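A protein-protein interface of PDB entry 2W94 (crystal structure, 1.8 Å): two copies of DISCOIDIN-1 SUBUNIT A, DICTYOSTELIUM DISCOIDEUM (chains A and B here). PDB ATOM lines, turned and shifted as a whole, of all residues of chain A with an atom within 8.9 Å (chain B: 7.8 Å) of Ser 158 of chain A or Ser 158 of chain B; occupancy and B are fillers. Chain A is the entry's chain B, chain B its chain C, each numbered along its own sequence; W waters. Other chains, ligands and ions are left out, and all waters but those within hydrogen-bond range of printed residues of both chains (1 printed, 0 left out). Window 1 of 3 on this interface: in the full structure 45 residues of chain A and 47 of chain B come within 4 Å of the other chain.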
ATOM      1  N   VAL A  68      15.244 -15.832  -8.954  1.00  0.00           N
ATOM      2  CA  VAL A  68      15.491 -16.814 -10.018  1.00  0.00           C
ATOM      3  C   VAL A  68      14.530 -17.980  -9.835  1.00  0.00           C
ATOM      4  O   VAL A  68      14.533 -18.668  -8.784  1.00  0.00           O
ATOM      5  CB  VAL A  68      16.910 -17.307  -9.983  1.00  0.00           C
ATOM      6  CG1 VAL A  68      17.142 -18.328 -11.144  1.00  0.00           C
ATOM      7  CG2 VAL A  68      17.862 -16.147 -10.105  1.00  0.00           C
ATOM      8  N   VAL A 155      20.161 -24.720  -9.941  1.00  0.00           N
ATOM      9  CA  VAL A 155      19.841 -23.827 -11.048  1.00  0.00           C
ATOM     10  C   VAL A 155      21.079 -23.562 -11.897  1.00  0.00           C
ATOM     11  O   VAL A 155      22.174 -23.583 -11.410  1.00  0.00           O
ATOM     12  CB  VAL A 155      19.294 -22.438 -10.572  1.00  0.00           C
ATOM     13  CG1 VAL A 155      17.962 -22.593  -9.929  1.00  0.00           C
ATOM     14  CG2 VAL A 155      20.282 -21.774  -9.694  1.00  0.00           C
ATOM     15  N   GLN A 156      20.876 -23.312 -13.177  1.00  0.00           N
ATOM     16  CA  GLN A 156      21.973 -22.851 -14.018  1.00  0.00           C
ATOM     17  C   GLN A 156      21.658 -21.438 -14.466  1.00  0.00           C
ATOM     18  O   GLN A 156      20.495 -21.082 -14.623  1.00  0.00           O
ATOM     19  CB  GLN A 156      22.171 -23.795 -15.194  1.00  0.00           C
ATOM     20  CG  GLN A 156      22.819 -25.120 -14.790  1.00  0.00           C
ATOM     21  CD  GLN A 156      21.779 -26.114 -14.348  1.00  0.00           C
ATOM     22  OE1 GLN A 156      20.602 -25.950 -14.678  1.00  0.00           O
ATOM     23  NE2 GLN A 156      22.185 -27.146 -13.569  1.00  0.00           N
ATOM     24  N   SER A 157      22.684 -20.625 -14.588  1.00  0.00           N
ATOM     25  CA  SER A 157      22.537 -19.258 -15.026  1.00  0.00           C
ATOM     26  C   SER A 157      23.322 -19.035 -16.312  1.00  0.00           C
ATOM     27  O   SER A 157      24.524 -19.332 -16.370  1.00  0.00           O
ATOM     28  CB  SER A 157      23.105 -18.338 -13.942  1.00  0.00           C
ATOM     29  OG  SER A 157      22.975 -16.994 -14.315  1.00  0.00           O
ATOM     30  N   SER A 158      22.683 -18.454 -17.328  1.00  0.00           N
ATOM     31  CA  SER A 158      23.378 -18.121 -18.544  1.00  0.00           C
ATOM     32  C   SER A 158      23.397 -16.644 -18.838  1.00  0.00           C
ATOM     33  O   SER A 158      22.463 -15.920 -18.498  1.00  0.00           O
ATOM     34  CB  SER A 158      22.741 -18.824 -19.752  1.00  0.00           C
ATOM     35  OG  SER A 158      21.358 -18.622 -19.819  1.00  0.00           O
ATOM     36  N   VAL A 159      24.434 -16.227 -19.525  1.00  0.00           N
ATOM     37  CA  VAL A 159      24.519 -14.870 -20.051  1.00  0.00           C
ATOM     38  C   VAL A 159      24.776 -14.956 -21.553  1.00  0.00           C
ATOM     39  O   VAL A 159      25.759 -15.562 -21.986  1.00  0.00           O
ATOM     40  CB  VAL A 159      25.585 -14.071 -19.369  1.00  0.00           C
ATOM     41  CG1 VAL A 159      25.659 -12.707 -19.996  1.00  0.00           C
ATOM     42  CG2 VAL A 159      25.263 -14.002 -17.855  1.00  0.00           C
ATOM     43  N   THR A 160      23.891 -14.383 -22.355  1.00  0.00           N
ATOM     44  CA  THR A 160      24.027 -14.524 -23.803  1.00  0.00           C
ATOM     45  C   THR A 160      24.278 -13.165 -24.469  1.00  0.00           C
ATOM     46  O   THR A 160      23.643 -12.161 -24.084  1.00  0.00           O
ATOM     47  CB  THR A 160      22.764 -15.176 -24.360  1.00  0.00           C
ATOM     48  OG1 THR A 160      22.609 -16.500 -23.844  1.00  0.00           O
ATOM     49  CG2 THR A 160      22.762 -15.181 -25.839  1.00  0.00           C
ATOM     50  N   GLN A 161      25.180 -13.124 -25.464  1.00  0.00           N
ATOM     51  CA  GLN A 161      25.378 -11.959 -26.338  1.00  0.00           C
ATOM     52  C   GLN A 161      25.154 -12.340 -27.805  1.00  0.00           C
ATOM     53  O   GLN A 161      25.601 -13.412 -28.271  1.00  0.00           O
ATOM     54  CB  GLN A 161      26.784 -11.382 -26.187  1.00  0.00           C
ATOM     55  CG  GLN A 161      27.017 -10.796 -24.773  1.00  0.00           C
ATOM     56  CD  GLN A 161      28.278 -10.097 -24.660  1.00  0.00           C
ATOM     57  OE1 GLN A 161      28.424  -9.025 -25.242  1.00  0.00           O
ATOM     58  NE2 GLN A 161      29.221 -10.664 -23.891  1.00  0.00           N
ATOM     59  N   VAL A 162      24.391 -11.494 -28.481  1.00  0.00           N
ATOM     60  CA  VAL A 162      24.108 -11.643 -29.907  1.00  0.00           C
ATOM     61  C   VAL A 162      24.913 -10.612 -30.624  1.00  0.00           C
ATOM     62  O   VAL A 162      24.981  -9.459 -30.209  1.00  0.00           O
ATOM     63  CB  VAL A 162      22.593 -11.497 -30.233  1.00  0.00           C
ATOM     64  CG1 VAL A 162      22.389 -11.154 -31.659  1.00  0.00           C
ATOM     65  CG2 VAL A 162      21.883 -12.736 -29.926  1.00  0.00           C
ATOM     66  N   PHE A 191      30.752  -6.852 -24.189  1.00  0.00           N
ATOM     67  CA  PHE A 191      31.379  -6.901 -22.847  1.00  0.00           C
ATOM     68  C   PHE A 191      32.044  -8.247 -22.649  1.00  0.00           C
ATOM     69  O   PHE A 191      31.658  -9.260 -23.259  1.00  0.00           O
ATOM     70  CB  PHE A 191      30.354  -6.603 -21.703  1.00  0.00           C
ATOM     71  CG  PHE A 191      29.244  -7.632 -21.570  1.00  0.00           C
ATOM     72  CD1 PHE A 191      29.447  -8.826 -20.881  1.00  0.00           C
ATOM     73  CD2 PHE A 191      28.015  -7.408 -22.146  1.00  0.00           C
ATOM     74  CE1 PHE A 191      28.428  -9.743 -20.773  1.00  0.00           C
ATOM     75  CE2 PHE A 191      27.017  -8.325 -22.056  1.00  0.00           C
ATOM     76  CZ  PHE A 191      27.202  -9.492 -21.367  1.00  0.00           C
ATOM     77  N   PHE A 193      32.833 -11.670 -21.045  1.00  0.00           N
ATOM     78  CA  PHE A 193      32.155 -12.704 -20.295  1.00  0.00           C
ATOM     79  C   PHE A 193      32.963 -13.006 -19.017  1.00  0.00           C
ATOM     80  O   PHE A 193      34.193 -12.841 -18.987  1.00  0.00           O
ATOM     81  CB  PHE A 193      32.017 -13.972 -21.140  1.00  0.00           C
ATOM     82  CG  PHE A 193      30.913 -13.929 -22.172  1.00  0.00           C
ATOM     83  CD1 PHE A 193      29.591 -13.951 -21.802  1.00  0.00           C
ATOM     84  CD2 PHE A 193      31.211 -13.905 -23.512  1.00  0.00           C
ATOM     85  CE1 PHE A 193      28.593 -13.920 -22.762  1.00  0.00           C
ATOM     86  CE2 PHE A 193      30.215 -13.843 -24.493  1.00  0.00           C
ATOM     87  CZ  PHE A 193      28.909 -13.898 -24.119  1.00  0.00           C
ATOM     88  N   THR A 195      33.043 -16.102 -17.725  1.00  0.00           N
ATOM     89  CA  THR A 195      33.652 -17.395 -17.926  1.00  0.00           C
ATOM     90  C   THR A 195      33.654 -17.646 -19.445  1.00  0.00           C
ATOM     91  O   THR A 195      33.017 -16.916 -20.202  1.00  0.00           O
ATOM     92  CB  THR A 195      32.896 -18.533 -17.238  1.00  0.00           C
ATOM     93  OG1 THR A 195      31.546 -18.547 -17.700  1.00  0.00           O
ATOM     94  CG2 THR A 195      32.886 -18.394 -15.703  1.00  0.00           C
ATOM     95  N   ALA A 250      26.603 -16.063 -28.507  1.00  0.00           N
ATOM     96  CA  ALA A 250      27.626 -16.543 -27.593  1.00  0.00           C
ATOM     97  C   ALA A 250      26.995 -16.616 -26.194  1.00  0.00           C
ATOM     98  O   ALA A 250      26.391 -15.641 -25.760  1.00  0.00           O
ATOM     99  CB  ALA A 250      28.777 -15.605 -27.597  1.00  0.00           C
ATOM    100  N   THR A 251      27.133 -17.749 -25.534  1.00  0.00           N
ATOM    101  CA  THR A 251      26.558 -17.937 -24.204  1.00  0.00           C
ATOM    102  C   THR A 251      27.587 -18.491 -23.230  1.00  0.00           C
ATOM    103  O   THR A 251      28.314 -19.448 -23.542  1.00  0.00           O
ATOM    104  CB  THR A 251      25.315 -18.889 -24.265  1.00  0.00           C
ATOM    105  OG1 THR A 251      24.306 -18.294 -25.067  1.00  0.00           O
ATOM    106  CG2 THR A 251      24.774 -19.173 -22.933  1.00  0.00           C
ATOM    107  N   ALA A 252      27.655 -17.849 -22.068  1.00  0.00           N
ATOM    108  CA  ALA A 252      28.454 -18.347 -20.966  1.00  0.00           C
ATOM    109  C   ALA A 252      27.569 -18.801 -19.821  1.00  0.00           C
ATOM    110  O   ALA A 252      26.554 -18.188 -19.499  1.00  0.00           O
ATOM    111  CB  ALA A 252      29.442 -17.268 -20.493  1.00  0.00           C
ATOM    112  N   LEU A 253      27.992 -19.864 -19.169  1.00  0.00           N
ATOM    113  CA  LEU A 253      27.226 -20.526 -18.113  1.00  0.00           C
ATOM    114  C   LEU A 253      27.917 -20.343 -16.755  1.00  0.00           C
ATOM    115  O   LEU A 253      29.141 -20.309 -16.666  1.00  0.00           O
ATOM    116  CB  LEU A 253      27.136 -22.022 -18.387  1.00  0.00           C
ATOM    117  CG  LEU A 253      26.208 -22.387 -19.544  1.00  0.00           C
ATOM    118  CD1 LEU A 253      26.296 -23.923 -19.780  1.00  0.00           C
ATOM    119  CD2 LEU A 253      24.838 -21.949 -19.205  1.00  0.00           C
ATOM    120  N   GLU A 254      27.109 -20.178 -15.715  1.00  0.00           N
ATOM    121  CA  GLU A 254      27.601 -20.168 -14.333  1.00  0.00           C
ATOM    122  C   GLU A 254      28.656 -19.097 -14.051  1.00  0.00           C
ATOM    123  O   GLU A 254      29.668 -19.263 -13.340  1.00  0.00           O
ATOM    124  CB  GLU A 254      28.053 -21.555 -13.978  1.00  0.00           C
ATOM    125  CG  GLU A 254      26.870 -22.547 -13.945  1.00  0.00           C
ATOM    126  CD  GLU A 254      25.911 -22.290 -12.776  1.00  0.00           C
ATOM    127  OE1 GLU A 254      26.145 -22.869 -11.674  1.00  0.00           O
ATOM    128  OE2 GLU A 254      24.912 -21.558 -12.945  1.00  0.00           O
ATOM    129  OXT GLU A 254      28.481 -17.980 -14.590  1.00  0.00           O
ATOM    130  N   VAL B  68      22.498 -14.895  -8.354  1.00  0.00           N
ATOM    131  CA  VAL B  68      23.221 -14.726  -9.619  1.00  0.00           C
ATOM    132  C   VAL B  68      24.729 -14.896  -9.338  1.00  0.00           C
ATOM    133  O   VAL B  68      25.308 -14.191  -8.541  1.00  0.00           O
ATOM    134  CB  VAL B  68      22.986 -13.309 -10.227  1.00  0.00           C
ATOM    135  CG1 VAL B  68      23.859 -13.097 -11.474  1.00  0.00           C
ATOM    136  CG2 VAL B  68      21.536 -13.082 -10.554  1.00  0.00           C
ATOM    137  N   PRO B  69      25.390 -15.846 -10.021  1.00  0.00           N
ATOM    138  CA  PRO B  69      26.803 -16.042  -9.746  1.00  0.00           C
ATOM    139  C   PRO B  69      27.657 -14.793  -9.931  1.00  0.00           C
ATOM    140  O   PRO B  69      27.428 -13.951 -10.829  1.00  0.00           O
ATOM    141  CB  PRO B  69      27.206 -17.188 -10.728  1.00  0.00           C
ATOM    142  CG  PRO B  69      25.927 -17.787 -11.133  1.00  0.00           C
ATOM    143  CD  PRO B  69      24.890 -16.736 -11.072  1.00  0.00           C
ATOM    144  N   ARG B 131      28.165 -18.337  -5.837  1.00  0.00           N
ATOM    145  CA  ARG B 131      26.886 -17.765  -5.453  1.00  0.00           C
ATOM    146  C   ARG B 131      26.913 -17.332  -4.002  1.00  0.00           C
ATOM    147  O   ARG B 131      26.497 -16.208  -3.672  1.00  0.00           O
ATOM    148  CB  ARG B 131      25.763 -18.765  -5.696  1.00  0.00           C
ATOM    149  CG  ARG B 131      25.329 -18.770  -7.201  1.00  0.00           C
ATOM    150  CD  ARG B 131      24.094 -19.599  -7.382  1.00  0.00           C
ATOM    151  NE  ARG B 131      23.555 -19.554  -8.754  1.00  0.00           N
ATOM    152  CZ  ARG B 131      23.962 -20.339  -9.749  1.00  0.00           C
ATOM    153  NH1 ARG B 131      24.915 -21.235  -9.547  1.00  0.00           N
ATOM    154  NH2 ARG B 131      23.412 -20.236 -10.952  1.00  0.00           N
ATOM    155  N   VAL B 155      27.974  -7.454 -12.765  1.00  0.00           N
ATOM    156  CA  VAL B 155      27.310  -8.515 -13.489  1.00  0.00           C
ATOM    157  C   VAL B 155      26.532  -7.956 -14.681  1.00  0.00           C
ATOM    158  O   VAL B 155      26.113  -6.783 -14.687  1.00  0.00           O
ATOM    159  CB  VAL B 155      26.345  -9.367 -12.615  1.00  0.00           C
ATOM    160  CG1 VAL B 155      27.074 -10.033 -11.495  1.00  0.00           C
ATOM    161  CG2 VAL B 155      25.244  -8.517 -12.046  1.00  0.00           C
ATOM    162  N   GLN B 156      26.304  -8.805 -15.669  1.00  0.00           N
ATOM    163  CA  GLN B 156      25.421  -8.452 -16.775  1.00  0.00           C
ATOM    164  C   GLN B 156      24.330  -9.509 -16.873  1.00  0.00           C
ATOM    165  O   GLN B 156      24.581 -10.683 -16.579  1.00  0.00           O
ATOM    166  CB  GLN B 156      26.183  -8.358 -18.101  1.00  0.00           C
ATOM    167  CG  GLN B 156      27.136  -7.225 -18.194  1.00  0.00           C
ATOM    168  CD  GLN B 156      28.496  -7.552 -17.602  1.00  0.00           C
ATOM    169  OE1 GLN B 156      28.885  -8.724 -17.483  1.00  0.00           O
ATOM    170  NE2 GLN B 156      29.220  -6.524 -17.214  1.00  0.00           N
ATOM    171  N   SER B 157      23.125  -9.087 -17.259  1.00  0.00           N
ATOM    172  CA  SER B 157      21.956  -9.915 -17.190  1.00  0.00           C
ATOM    173  C   SER B 157      21.303  -9.916 -18.591  1.00  0.00           C
ATOM    174  O   SER B 157      21.023  -8.857 -19.128  1.00  0.00           O
ATOM    175  CB  SER B 157      20.966  -9.364 -16.162  1.00  0.00           C
ATOM    176  OG  SER B 157      19.866 -10.251 -16.081  1.00  0.00           O
ATOM    177  N   SER B 158      21.055 -11.097 -19.151  1.00  0.00           N
ATOM    178  CA  SER B 158      20.416 -11.204 -20.482  1.00  0.00           C
ATOM    179  C   SER B 158      19.095 -11.950 -20.421  1.00  0.00           C
ATOM    180  O   SER B 158      18.919 -12.828 -19.603  1.00  0.00           O
ATOM    181  CB  SER B 158      21.359 -11.909 -21.472  1.00  0.00           C
ATOM    182  OG  SER B 158      21.652 -13.197 -21.037  1.00  0.00           O
ATOM    183  N   VAL B 159      18.155 -11.598 -21.306  1.00  0.00           N
ATOM    184  CA  VAL B 159      16.932 -12.403 -21.503  1.00  0.00           C
ATOM    185  C   VAL B 159      16.841 -12.764 -22.993  1.00  0.00           C
ATOM    186  O   VAL B 159      16.969 -11.895 -23.838  1.00  0.00           O
ATOM    187  CB  VAL B 159      15.649 -11.648 -21.132  1.00  0.00           C
ATOM    188  CG1 VAL B 159      14.397 -12.561 -21.387  1.00  0.00           C
ATOM    189  CG2 VAL B 159      15.681 -11.202 -19.648  1.00  0.00           C
ATOM    190  N   THR B 160      16.737 -14.046 -23.293  1.00  0.00           N
ATOM    191  CA  THR B 160      16.797 -14.502 -24.685  1.00  0.00           C
ATOM    192  C   THR B 160      15.492 -15.195 -25.046  1.00  0.00           C
ATOM    193  O   THR B 160      14.962 -15.976 -24.223  1.00  0.00           O
ATOM    194  CB  THR B 160      17.957 -15.456 -24.871  1.00  0.00           C
ATOM    195  OG1 THR B 160      19.179 -14.776 -24.530  1.00  0.00           O
ATOM    196  CG2 THR B 160      18.023 -16.021 -26.278  1.00  0.00           C
ATOM    197  N   GLN B 161      14.977 -14.941 -26.268  1.00  0.00           N
ATOM    198  CA  GLN B 161      13.836 -15.701 -26.793  1.00  0.00           C
ATOM    199  C   GLN B 161      14.242 -16.326 -28.151  1.00  0.00           C
ATOM    200  O   GLN B 161      14.809 -15.639 -29.013  1.00  0.00           O
ATOM    201  CB  GLN B 161      12.606 -14.826 -27.036  1.00  0.00           C
ATOM    202  CG  GLN B 161      12.011 -14.232 -25.738  1.00  0.00           C
ATOM    203  CD  GLN B 161      10.822 -13.374 -25.977  1.00  0.00           C
ATOM    204  OE1 GLN B 161       9.770 -13.877 -26.358  1.00  0.00           O
ATOM    205  NE2 GLN B 161      10.963 -12.058 -25.738  1.00  0.00           N
ATOM    206  N   PHE B 193      10.082  -7.589 -24.634  1.00  0.00           N
ATOM    207  CA  PHE B 193      11.341  -7.415 -23.918  1.00  0.00           C
ATOM    208  C   PHE B 193      11.303  -6.092 -23.115  1.00  0.00           C
ATOM    209  O   PHE B 193      10.696  -5.110 -23.545  1.00  0.00           O
ATOM    210  CB  PHE B 193      12.522  -7.343 -24.897  1.00  0.00           C
ATOM    211  CG  PHE B 193      12.981  -8.677 -25.470  1.00  0.00           C
ATOM    212  CD1 PHE B 193      13.717  -9.553 -24.711  1.00  0.00           C
ATOM    213  CD2 PHE B 193      12.743  -8.994 -26.794  1.00  0.00           C
ATOM    214  CE1 PHE B 193      14.190 -10.767 -25.265  1.00  0.00           C
ATOM    215  CE2 PHE B 193      13.154 -10.211 -27.329  1.00  0.00           C
ATOM    216  CZ  PHE B 193      13.910 -11.073 -26.593  1.00  0.00           C
ATOM    217  N   ALA B 250      16.751 -13.749 -30.270  1.00  0.00           N
ATOM    218  CA  ALA B 250      16.688 -12.351 -29.853  1.00  0.00           C
ATOM    219  C   ALA B 250      17.097 -12.258 -28.356  1.00  0.00           C
ATOM    220  O   ALA B 250      16.545 -12.997 -27.529  1.00  0.00           O
ATOM    221  CB  ALA B 250      15.290 -11.822 -30.022  1.00  0.00           C
ATOM    222  N   THR B 251      18.026 -11.358 -28.040  1.00  0.00           N
ATOM    223  CA  THR B 251      18.523 -11.192 -26.692  1.00  0.00           C
ATOM    224  C   THR B 251      18.517  -9.710 -26.321  1.00  0.00           C
ATOM    225  O   THR B 251      18.990  -8.878 -27.077  1.00  0.00           O
ATOM    226  CB  THR B 251      19.949 -11.770 -26.552  1.00  0.00           C
ATOM    227  OG1 THR B 251      19.895 -13.191 -26.803  1.00  0.00           O
ATOM    228  CG2 THR B 251      20.436 -11.548 -25.137  1.00  0.00           C
ATOM    229  N   ALA B 252      17.986  -9.407 -25.137  1.00  0.00           N
ATOM    230  CA  ALA B 252      18.041  -8.058 -24.578  1.00  0.00           C
ATOM    231  C   ALA B 252      18.907  -8.055 -23.286  1.00  0.00           C
ATOM    232  O   ALA B 252      18.939  -9.042 -22.537  1.00  0.00           O
ATOM    233  CB  ALA B 252      16.665  -7.548 -24.302  1.00  0.00           C
ATOM    234  N   LEU B 253      19.632  -6.961 -23.066  1.00  0.00           N
ATOM    235  CA  LEU B 253      20.636  -6.854 -21.990  1.00  0.00           C
ATOM    236  C   LEU B 253      20.176  -5.861 -20.905  1.00  0.00           C
ATOM    237  O   LEU B 253      19.523  -4.856 -21.202  1.00  0.00           O
ATOM    238  CB  LEU B 253      21.992  -6.385 -22.526  1.00  0.00           C
ATOM    239  CG  LEU B 253      22.824  -7.298 -23.429  1.00  0.00           C
ATOM    240  CD1 LEU B 253      24.143  -6.611 -23.747  1.00  0.00           C
ATOM    241  CD2 LEU B 253      23.035  -8.590 -22.751  1.00  0.00           C
ATOM    242  N   GLU B 254      20.476  -6.208 -19.659  1.00  0.00           N
ATOM    243  CA  GLU B 254      20.188  -5.381 -18.497  1.00  0.00           C
ATOM    244  C   GLU B 254      18.699  -4.987 -18.388  1.00  0.00           C
ATOM    245  O   GLU B 254      18.331  -3.801 -18.147  1.00  0.00           O
ATOM    246  CB  GLU B 254      21.118  -4.166 -18.517  1.00  0.00           C
ATOM    247  CG  GLU B 254      22.593  -4.573 -18.295  1.00  0.00           C
ATOM    248  CD  GLU B 254      22.900  -4.996 -16.843  1.00  0.00           C
ATOM    249  OE1 GLU B 254      23.249  -4.113 -16.028  1.00  0.00           O
ATOM    250  OE2 GLU B 254      22.827  -6.189 -16.563  1.00  0.00           O
ATOM    251  OXT GLU B 254      17.817  -5.858 -18.553  1.00  0.00           O
HETATM  252  O   HOH W   1      21.333 -13.604 -17.731  1.00  0.00           O
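Of the printed residues of chain B, Val 155 of chain A touches Arg 131 (3.6 Å).
Ser 157 of chain A touches just these residues of chain B: Pro 69 (3.7 Å) and Arg 131 (3.6 Å).
Of the printed residues of chain B, Val 159 of chain A touches Gln 156 and Ser 158.
Of the printed residues of chain B, Val 162 of chain A touches Thr 251.
Of the printed residues of chain A, Pro 69 of chain B touches Ser 157 (3.7 Å).
Printed residues of chain A within 4 Å of Arg 131 of chain B: Val 155, Ser 157 and Glu 254.
No residue of chain A comes within 4 Å of Ser 157 of chain B.
Ser 158 of chain B touches just these residues of chain A: Ser 158 (3.8 Å), Val 159 (3.5 Å) and Thr 160 (2.9 Å).
The nearest residue of chain B that does not touch Ser 158 of chain A is Gln 156 of chain B (6.0 Å).
The nearest residue of chain A that does not touch Ser 158 of chain B is Gln 161 of chain A (5.7 Å).
Along chain A the printed residues that touch a printed residue of chain B span positions 155 to 254.
Of the 16 printed residues of chain B, 7 touch a printed residue of chain A.
Hydrophobic or aromatic side chains of chain B within 4 Å of the printed part of chain A: Pro 69 and Leu 253.
Among the printed residues, 14 pairs touch across the chains.
Among the printed residues, Asp or Glu carboxylates within 4 Å of a Lys or Arg side-chain nitrogen of the other chain: Glu 254 of chain A with Arg 131 of chain B.
Val 159 of chain A touches Gln 156 of chain B, but with the chains exchanged Gln 156 of chain A does not touch Val 159 of chain B (11.6 Å).
Thr 160 of chain B touches its own counterpart, Thr 160 of chain A.
Thr 160 of chain A touches Thr 251 of chain B, but with the chains exchanged Thr 251 of chain A does not touch Thr 160 of chain B (6.2 Å).
Thr 160 of chain A touches Leu 253 of chain B, but with the chains exchanged Leu 253 of chain A does not touch Thr 160 of chain B (10.6 Å).
Of the 14 pairs that touch across the chains among the printed residues, 2 have their exchanged pair printed and touching as well.
Val 155 of chain A touches Arg 131 of chain B (O to NH2, 3.6 Å).
CB of Ser 157 of chain A touches CD of Pro 69 of chain B (3.7 Å).
Ser 158 of chain B touches Ser 158 of chain A.
CA of Val 159 of chain A touches OG of Ser 158 of chain B, 3.5 Å away.
Thr 160 of chain A touches Thr 160 of chain B (CB to OG1, 3.6 Å).
Thr 160 of chain A touches Thr 251 of chain B.
CD2 of Leu 253 of chain B touches O of Thr 160 of chain A, 3.9 Å away.
OG1 of Thr 251 of chain B touches CG2 of Val 162 of chain A, 3.7 Å away.
Gln 156 of chain B touches Phe 191 of chain A.
CE2 of Phe 191 of chain A touches CD1 of Leu 253 of chain B, at 3.7 Å.
Water W1 bridges O of Ser 158 of chain A and N of Ser 158 of chain B.
The side-chain carboxylate (OE2) of Glu 254 of chain A lies within salt-bridge range of the guanidinium group (NH2) of Arg 131 of chain B, at 2.8 Å.
The side-chain hydroxyl (OG) of Ser 158 of chain B sits at hydrogen-bond distance from the backbone NH (N) of Thr 160 of chain A.
The backbone carbonyl oxygen (O) of Ala 252 of chain A is in hydrogen-bond range of the backbone NH (N) of Val 159 of chain A, at 2.9 Å.
OG1 of Thr 160 of chain B sits at hydrogen-bond distance from OG1 of Thr 251 of chain B (2.9 Å).
The backbone NH of Glu 254 of chain A lies within hydrogen-bond range of the backbone carbonyl oxygen of Ser 157 of chain A (2.8 Å).
The side-chain hydroxyl of Thr 160 of chain A sits at hydrogen-bond distance from the side-chain hydroxyl of Thr 251 of chain A (2.8 Å).
NE2 of Gln 161 of chain A sits at hydrogen-bond distance from O of Phe 191 of chain A, at 2.9 Å.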
